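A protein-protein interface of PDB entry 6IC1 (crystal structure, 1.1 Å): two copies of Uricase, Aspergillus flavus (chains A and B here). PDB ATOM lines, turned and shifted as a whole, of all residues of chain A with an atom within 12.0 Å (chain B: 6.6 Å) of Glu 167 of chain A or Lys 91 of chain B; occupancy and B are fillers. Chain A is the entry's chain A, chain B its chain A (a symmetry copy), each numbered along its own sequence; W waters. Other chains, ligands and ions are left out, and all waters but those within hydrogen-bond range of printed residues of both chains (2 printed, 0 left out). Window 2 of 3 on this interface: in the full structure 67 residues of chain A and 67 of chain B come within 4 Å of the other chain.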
ATOM      1  N   PHE A 163       8.787  29.965 -14.446  1.00  0.00           N
ATOM      2  CA  PHE A 163       8.550  29.750 -13.036  1.00  0.00           C
ATOM      3  C   PHE A 163       7.073  29.563 -12.736  1.00  0.00           C
ATOM      4  O   PHE A 163       6.183  29.836 -13.569  1.00  0.00           O
ATOM      5  CB  PHE A 163       9.176  30.888 -12.236  1.00  0.00           C
ATOM      6  CG  PHE A 163       8.722  32.250 -12.655  1.00  0.00           C
ATOM      7  CD1 PHE A 163       7.579  32.837 -12.127  1.00  0.00           C
ATOM      8  CD2 PHE A 163       9.469  32.950 -13.585  1.00  0.00           C
ATOM      9  CE1 PHE A 163       7.201  34.105 -12.559  1.00  0.00           C
ATOM     10  CE2 PHE A 163       9.089  34.216 -14.019  1.00  0.00           C
ATOM     11  CZ  PHE A 163       7.956  34.775 -13.512  1.00  0.00           C
ATOM     12  N   LEU A 164       6.773  29.019 -11.579  1.00  0.00           N
ATOM     13  CA  LEU A 164       5.409  28.731 -11.141  1.00  0.00           C
ATOM     14  C   LEU A 164       4.592  30.015 -11.134  1.00  0.00           C
ATOM     15  O   LEU A 164       5.036  31.029 -10.621  1.00  0.00           O
ATOM     16  CB  LEU A 164       5.449  28.041  -9.771  1.00  0.00           C
ATOM     17  CG  LEU A 164       4.125  27.487  -9.259  1.00  0.00           C
ATOM     18  CD1 LEU A 164       4.375  26.333  -8.313  1.00  0.00           C
ATOM     19  CD2 LEU A 164       3.338  28.580  -8.549  1.00  0.00           C
ATOM     20  N   ARG A 165       3.382  29.938 -11.666  1.00  0.00           N
ATOM     21  CA  ARG A 165       2.465  31.069 -11.750  1.00  0.00           C
ATOM     22  C   ARG A 165       1.165  30.671 -11.093  1.00  0.00           C
ATOM     23  O   ARG A 165       0.492  29.728 -11.587  1.00  0.00           O
ATOM     24  CB  ARG A 165       2.140  31.472 -13.191  1.00  0.00           C
ATOM     25  CG  ARG A 165       3.374  31.772 -14.007  1.00  0.00           C
ATOM     26  CD  ARG A 165       3.134  32.568 -15.295  1.00  0.00           C
ATOM     27  NE  ARG A 165       2.803  33.869 -15.005  1.00  0.00           N
ATOM     28  CZ  ARG A 165       3.582  34.876 -14.696  1.00  0.00           C
ATOM     29  NH1 ARG A 165       4.880  34.732 -14.855  1.00  0.00           N
ATOM     30  NH2 ARG A 165       3.029  35.978 -14.293  1.00  0.00           N
ATOM     31  N   ASP A 166       0.756  31.369 -10.067  1.00  0.00           N
ATOM     32  CA  ASP A 166      -0.534  31.149  -9.402  1.00  0.00           C
ATOM     33  C   ASP A 166      -1.077  32.480  -8.933  1.00  0.00           C
ATOM     34  O   ASP A 166      -0.625  33.562  -9.376  1.00  0.00           O
ATOM     35  CB  ASP A 166      -0.406  30.103  -8.316  1.00  0.00           C
ATOM     36  CG  ASP A 166       0.424  30.537  -7.104  1.00  0.00           C
ATOM     37  OD1 ASP A 166       0.820  31.721  -7.067  1.00  0.00           O
ATOM     38  OD2 ASP A 166       0.638  29.665  -6.225  1.00  0.00           O
ATOM     39  N   GLU A 167      -2.040  32.465  -8.025  1.00  0.00           N
ATOM     40  CA  GLU A 167      -2.729  33.671  -7.605  1.00  0.00           C
ATOM     41  C   GLU A 167      -1.841  34.600  -6.763  1.00  0.00           C
ATOM     42  O   GLU A 167      -2.308  35.694  -6.455  1.00  0.00           O
ATOM     43  CB  GLU A 167      -4.029  33.323  -6.845  1.00  0.00           C
ATOM     44  CG  GLU A 167      -3.898  32.545  -5.543  1.00  0.00           C
ATOM     45  CD  GLU A 167      -3.788  31.017  -5.653  1.00  0.00           C
ATOM     46  OE1 GLU A 167      -3.450  30.507  -6.697  1.00  0.00           O
ATOM     47  OE2 GLU A 167      -4.049  30.383  -4.583  1.00  0.00           O
ATOM     48  N   TYR A 168      -0.646  34.169  -6.395  1.00  0.00           N
ATOM     49  CA  TYR A 168       0.304  35.035  -5.665  1.00  0.00           C
ATOM     50  C   TYR A 168       1.322  35.667  -6.630  1.00  0.00           C
ATOM     51  O   TYR A 168       2.170  36.449  -6.132  1.00  0.00           O
ATOM     52  CB  TYR A 168       1.027  34.220  -4.594  1.00  0.00           C
ATOM     53  CG  TYR A 168       0.079  33.698  -3.527  1.00  0.00           C
ATOM     54  CD1 TYR A 168      -0.225  34.451  -2.384  1.00  0.00           C
ATOM     55  CD2 TYR A 168      -0.532  32.443  -3.633  1.00  0.00           C
ATOM     56  CE1 TYR A 168      -1.103  34.024  -1.424  1.00  0.00           C
ATOM     57  CE2 TYR A 168      -1.398  32.028  -2.685  1.00  0.00           C
ATOM     58  CZ  TYR A 168      -1.716  32.794  -1.596  1.00  0.00           C
ATOM     59  OH  TYR A 168      -2.609  32.358  -0.632  1.00  0.00           O
ATOM     60  N   THR A 169       1.241  35.382  -7.917  1.00  0.00           N
ATOM     61  CA  THR A 169       2.291  35.755  -8.853  1.00  0.00           C
ATOM     62  C   THR A 169       1.916  37.031  -9.614  1.00  0.00           C
ATOM     63  O   THR A 169       0.878  37.044 -10.283  1.00  0.00           O
ATOM     64  CB  THR A 169       2.563  34.636  -9.860  1.00  0.00           C
ATOM     65  OG1 THR A 169       2.721  33.389  -9.170  1.00  0.00           O
ATOM     66  CG2 THR A 169       3.756  34.901 -10.742  1.00  0.00           C
ATOM     67  N   THR A 170       2.784  38.013  -9.589  1.00  0.00           N
ATOM     68  CA  THR A 170       2.721  39.202 -10.446  1.00  0.00           C
ATOM     69  C   THR A 170       3.914  39.301 -11.386  1.00  0.00           C
ATOM     70  O   THR A 170       3.845  40.053 -12.372  1.00  0.00           O
ATOM     71  CB  THR A 170       2.593  40.474  -9.623  1.00  0.00           C
ATOM     72  OG1 THR A 170       3.715  40.529  -8.733  1.00  0.00           O
ATOM     73  CG2 THR A 170       1.327  40.514  -8.830  1.00  0.00           C
ATOM     74  N   LEU A 171       5.015  38.629 -11.103  1.00  0.00           N
ATOM     75  CA  LEU A 171       6.248  38.832 -11.845  1.00  0.00           C
ATOM     76  C   LEU A 171       6.090  38.457 -13.311  1.00  0.00           C
ATOM     77  O   LEU A 171       5.686  37.320 -13.617  1.00  0.00           O
ATOM     78  CB  LEU A 171       7.346  37.971 -11.224  1.00  0.00           C
ATOM     79  CG  LEU A 171       8.742  38.107 -11.835  1.00  0.00           C
ATOM     80  CD1 LEU A 171       9.301  39.520 -11.673  1.00  0.00           C
ATOM     81  CD2 LEU A 171       9.703  37.095 -11.254  1.00  0.00           C
ATOM     82  N   ILE B  67       0.528  39.893   1.668  1.00  0.00           N
ATOM     83  CA  ILE B  67      -0.836  39.341   1.738  1.00  0.00           C
ATOM     84  C   ILE B  67      -1.104  38.722   3.101  1.00  0.00           C
ATOM     85  O   ILE B  67      -2.151  38.920   3.711  1.00  0.00           O
ATOM     86  CB  ILE B  67      -1.062  38.372   0.599  1.00  0.00           C
ATOM     87  CG1 ILE B  67      -1.098  39.095  -0.729  1.00  0.00           C
ATOM     88  CG2 ILE B  67      -2.337  37.533   0.816  1.00  0.00           C
ATOM     89  CD1 ILE B  67      -0.845  38.208  -1.948  1.00  0.00           C
ATOM     90  N   THR B  86       3.771  28.048   7.525  1.00  0.00           N
ATOM     91  CA  THR B  86       2.774  26.984   7.298  1.00  0.00           C
ATOM     92  C   THR B  86       2.138  27.180   5.926  1.00  0.00           C
ATOM     93  O   THR B  86       1.892  26.187   5.220  1.00  0.00           O
ATOM     94  CB  THR B  86       1.736  26.999   8.415  1.00  0.00           C
ATOM     95  OG1 THR B  86       2.373  26.636   9.649  1.00  0.00           O
ATOM     96  CG2 THR B  86       0.586  26.042   8.171  1.00  0.00           C
ATOM     97  N   HIS B  87       1.887  28.418   5.525  1.00  0.00           N
ATOM     98  CA  HIS B  87       1.266  28.688   4.219  1.00  0.00           C
ATOM     99  C   HIS B  87       2.079  28.033   3.110  1.00  0.00           C
ATOM    100  O   HIS B  87       1.524  27.353   2.254  1.00  0.00           O
ATOM    101  CB  HIS B  87       1.182  30.160   3.966  1.00  0.00           C
ATOM    102  CG  HIS B  87       0.884  30.454   2.555  1.00  0.00           C
ATOM    103  ND1 HIS B  87      -0.345  30.289   1.969  1.00  0.00           N
ATOM    104  CD2 HIS B  87       1.765  30.782   1.573  1.00  0.00           C
ATOM    105  CE1 HIS B  87      -0.170  30.549   0.718  1.00  0.00           C
ATOM    106  NE2 HIS B  87       1.051  30.870   0.392  1.00  0.00           N
ATOM    107  N   PHE B  88       3.412  28.219   3.111  1.00  0.00           N
ATOM    108  CA  PHE B  88       4.174  27.718   1.966  1.00  0.00           C
ATOM    109  C   PHE B  88       4.221  26.196   1.927  1.00  0.00           C
ATOM    110  O   PHE B  88       4.160  25.692   0.859  1.00  0.00           O
ATOM    111  CB  PHE B  88       5.603  28.269   2.008  1.00  0.00           C
ATOM    112  CG  PHE B  88       5.643  29.748   1.691  1.00  0.00           C
ATOM    113  CD1 PHE B  88       5.468  30.191   0.391  1.00  0.00           C
ATOM    114  CD2 PHE B  88       5.821  30.690   2.677  1.00  0.00           C
ATOM    115  CE1 PHE B  88       5.488  31.535   0.090  1.00  0.00           C
ATOM    116  CE2 PHE B  88       5.816  32.060   2.395  1.00  0.00           C
ATOM    117  CZ  PHE B  88       5.681  32.474   1.081  1.00  0.00           C
ATOM    118  N   ILE B  89       4.342  25.509   3.028  1.00  0.00           N
ATOM    119  CA  ILE B  89       4.414  24.053   2.949  1.00  0.00           C
ATOM    120  C   ILE B  89       3.029  23.483   2.661  1.00  0.00           C
ATOM    121  O   ILE B  89       2.966  22.366   2.107  1.00  0.00           O
ATOM    122  CB  ILE B  89       5.061  23.406   4.182  1.00  0.00           C
ATOM    123  CG1 ILE B  89       4.313  23.599   5.481  1.00  0.00           C
ATOM    124  CG2 ILE B  89       6.500  23.848   4.373  1.00  0.00           C
ATOM    125  CD1 ILE B  89       4.583  22.520   6.485  1.00  0.00           C
ATOM    126  N   GLU B  90       1.936  24.148   3.049  1.00  0.00           N
ATOM    127  CA  GLU B  90       0.567  23.637   2.762  1.00  0.00           C
ATOM    128  C   GLU B  90       0.192  23.951   1.315  1.00  0.00           C
ATOM    129  O   GLU B  90      -0.444  23.141   0.641  1.00  0.00           O
ATOM    130  CB  GLU B  90      -0.435  24.185   3.747  1.00  0.00           C
ATOM    131  CG  GLU B  90      -0.288  23.647   5.108  1.00  0.00           C
ATOM    132  CD  GLU B  90      -1.375  24.008   6.090  1.00  0.00           C
ATOM    133  OE1 GLU B  90      -2.155  24.985   5.805  1.00  0.00           O
ATOM    134  OE2 GLU B  90      -1.402  23.393   7.202  1.00  0.00           O
ATOM    135  N   LYS B  91       0.515  25.162   0.859  1.00  0.00           N
ATOM    136  CA  LYS B  91       0.054  25.602  -0.479  1.00  0.00           C
ATOM    137  C   LYS B  91       0.764  24.796  -1.578  1.00  0.00           C
ATOM    138  O   LYS B  91       0.143  24.546  -2.631  1.00  0.00           O
ATOM    139  CB  LYS B  91       0.291  27.086  -0.644  1.00  0.00           C
ATOM    140  CG  LYS B  91      -0.131  27.657  -1.991  1.00  0.00           C
ATOM    141  CD  LYS B  91      -1.635  27.486  -2.260  1.00  0.00           C
ATOM    142  CE  LYS B  91      -1.977  28.016  -3.615  1.00  0.00           C
ATOM    143  NZ  LYS B  91      -3.426  27.740  -3.913  1.00  0.00           N
ATOM    144  N   TYR B  92       2.055  24.517  -1.428  1.00  0.00           N
ATOM    145  CA  TYR B  92       2.863  23.960  -2.480  1.00  0.00           C
ATOM    146  C   TYR B  92       3.252  22.545  -2.071  1.00  0.00           C
ATOM    147  O   TYR B  92       4.035  22.347  -1.112  1.00  0.00           O
ATOM    148  CB  TYR B  92       4.097  24.819  -2.755  1.00  0.00           C
ATOM    149  CG  TYR B  92       3.722  26.201  -3.189  1.00  0.00           C
ATOM    150  CD1 TYR B  92       3.167  26.436  -4.417  1.00  0.00           C
ATOM    151  CD2 TYR B  92       3.800  27.290  -2.317  1.00  0.00           C
ATOM    152  CE1 TYR B  92       2.755  27.696  -4.825  1.00  0.00           C
ATOM    153  CE2 TYR B  92       3.381  28.555  -2.701  1.00  0.00           C
ATOM    154  CZ  TYR B  92       2.819  28.772  -3.939  1.00  0.00           C
ATOM    155  OH  TYR B  92       2.382  30.010  -4.280  1.00  0.00           O
ATOM    156  N   ASN B  93       2.754  21.549  -2.790  1.00  0.00           N
ATOM    157  CA  ASN B  93       3.016  20.166  -2.408  1.00  0.00           C
ATOM    158  C   ASN B  93       4.526  19.923  -2.341  1.00  0.00           C
ATOM    159  O   ASN B  93       4.988  19.215  -1.412  1.00  0.00           O
ATOM    160  CB  ASN B  93       2.335  19.195  -3.371  1.00  0.00           C
ATOM    161  CG  ASN B  93       0.850  19.162  -3.210  1.00  0.00           C
ATOM    162  OD1 ASN B  93       0.262  19.642  -2.243  1.00  0.00           O
ATOM    163  ND2 ASN B  93       0.237  18.479  -4.148  1.00  0.00           N
ATOM    164  N   HIS B  94       5.279  20.459  -3.273  1.00  0.00           N
ATOM    165  CA  HIS B  94       6.706  20.135  -3.438  1.00  0.00           C
ATOM    166  C   HIS B  94       7.630  20.949  -2.521  1.00  0.00           C
ATOM    167  O   HIS B  94       8.820  20.718  -2.507  1.00  0.00           O
ATOM    168  CB  HIS B  94       7.160  20.293  -4.873  1.00  0.00           C
ATOM    169  CG  HIS B  94       7.310  21.681  -5.353  1.00  0.00           C
ATOM    170  ND1 HIS B  94       6.246  22.579  -5.412  1.00  0.00           N
ATOM    171  CD2 HIS B  94       8.412  22.354  -5.722  1.00  0.00           C
ATOM    172  CE1 HIS B  94       6.722  23.727  -5.892  1.00  0.00           C
ATOM    173  NE2 HIS B  94       8.062  23.641  -6.021  1.00  0.00           N
HETATM  174  O   HOH W   1      -3.250  27.823  -6.742  1.00  0.00           O
HETATM  175  O   HOH W   2       3.502  31.800  -6.358  1.00  0.00           O
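The side-chain carboxylate (OD1) of Asp 166 of chain A is in hydrogen-bond range of the backbone NH (N) of Tyr 168 of chain A. OG1 of Thr 169 of chain A lies within hydrogen-bond range of N of Asp 166 of chain A.
OE2 of Glu 167 of chain A lies within salt-bridge range of NZ of Lys 91 of chain B (2.8 Å). OH of Tyr 92 of chain B sits at hydrogen-bond distance from OD2 of Asp 166 of chain A (2.6 Å).
No position is printed for both chains. Of the 6 pairs that touch across the chains among the printed residues, none has its exchanged pair printed and touching as well.
Water W1 bridges the side-chain carboxylate of Glu 167 of chain A (2.7 Å) and the side-chain amino group of Lys 91 of chain B (2.8 Å). Water W2 lies within hydrogen-bond range of OD1 of Asp 166 of chain A (2.8 Å), OH of Tyr 92 of chain B (3.0 Å) and OG1 of Thr 169 of chain A (3.3 Å).
CD2 of Leu 164 of chain A touches CE1 of Tyr 92 of chain B (3.9 Å). Ile 67 of chain B touches Tyr 168 of chain A (CD1 to CD1, 3.8 Å). CE1 of His 87 of chain B touches OH of Tyr 168 of chain A, at 3.3 Å. Tyr 92 of chain B touches Tyr 168 of chain A (OH to CD2, 3.9 Å).
Of the 9 printed residues of chain A, 4 touch a printed residue of chain B. Printed residues of chain A that touch a printed residue of chain B: Leu 164, Asp 166, Glu 167 and Tyr 168. Hydrophobic or aromatic side chains of chain A within 4 Å of the printed part of chain B: Leu 164 and Tyr 168. Hydrophobic or aromatic side chains of chain B within 4 Å of the printed part of chain A: Ile 67, His 87 and Tyr 92. Among the printed residues, 6 pairs touch across the chains.
Glu 167 of chain A touches just one residue of chain B: Lys 91 (2.8 Å). Of chain A, only Glu 167 comes within 4 Å of Lys 91 of chain B. His 87 of chain B touches just one residue of chain A: Tyr 168 (3.3 Å). No residue of chain A comes within 4 Å of Ile 89 of chain B. Asn 93 of chain B touches none of the printed residues of chain A. Of the printed residues of chain B, Leu 164 of chain A touches Tyr 92 (3.9 Å). Printed residues of chain B within 4 Å of Tyr 168 of chain A: Ile 67, His 87 and Tyr 92. Printed residues of chain A within 4 Å of Ile 67 of chain B: Tyr 168. Of the printed residues of chain B, Asp 166 of chain A touches Tyr 92 (2.6 Å). Arg 165 of chain A touches none of the printed residues of chain B. Thr 86 of chain B touches none of the printed residues of chain A. The nearest residue of chain A that does not touch Lys 91 of chain B is Asp 166 of chain A (4.05 Å).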
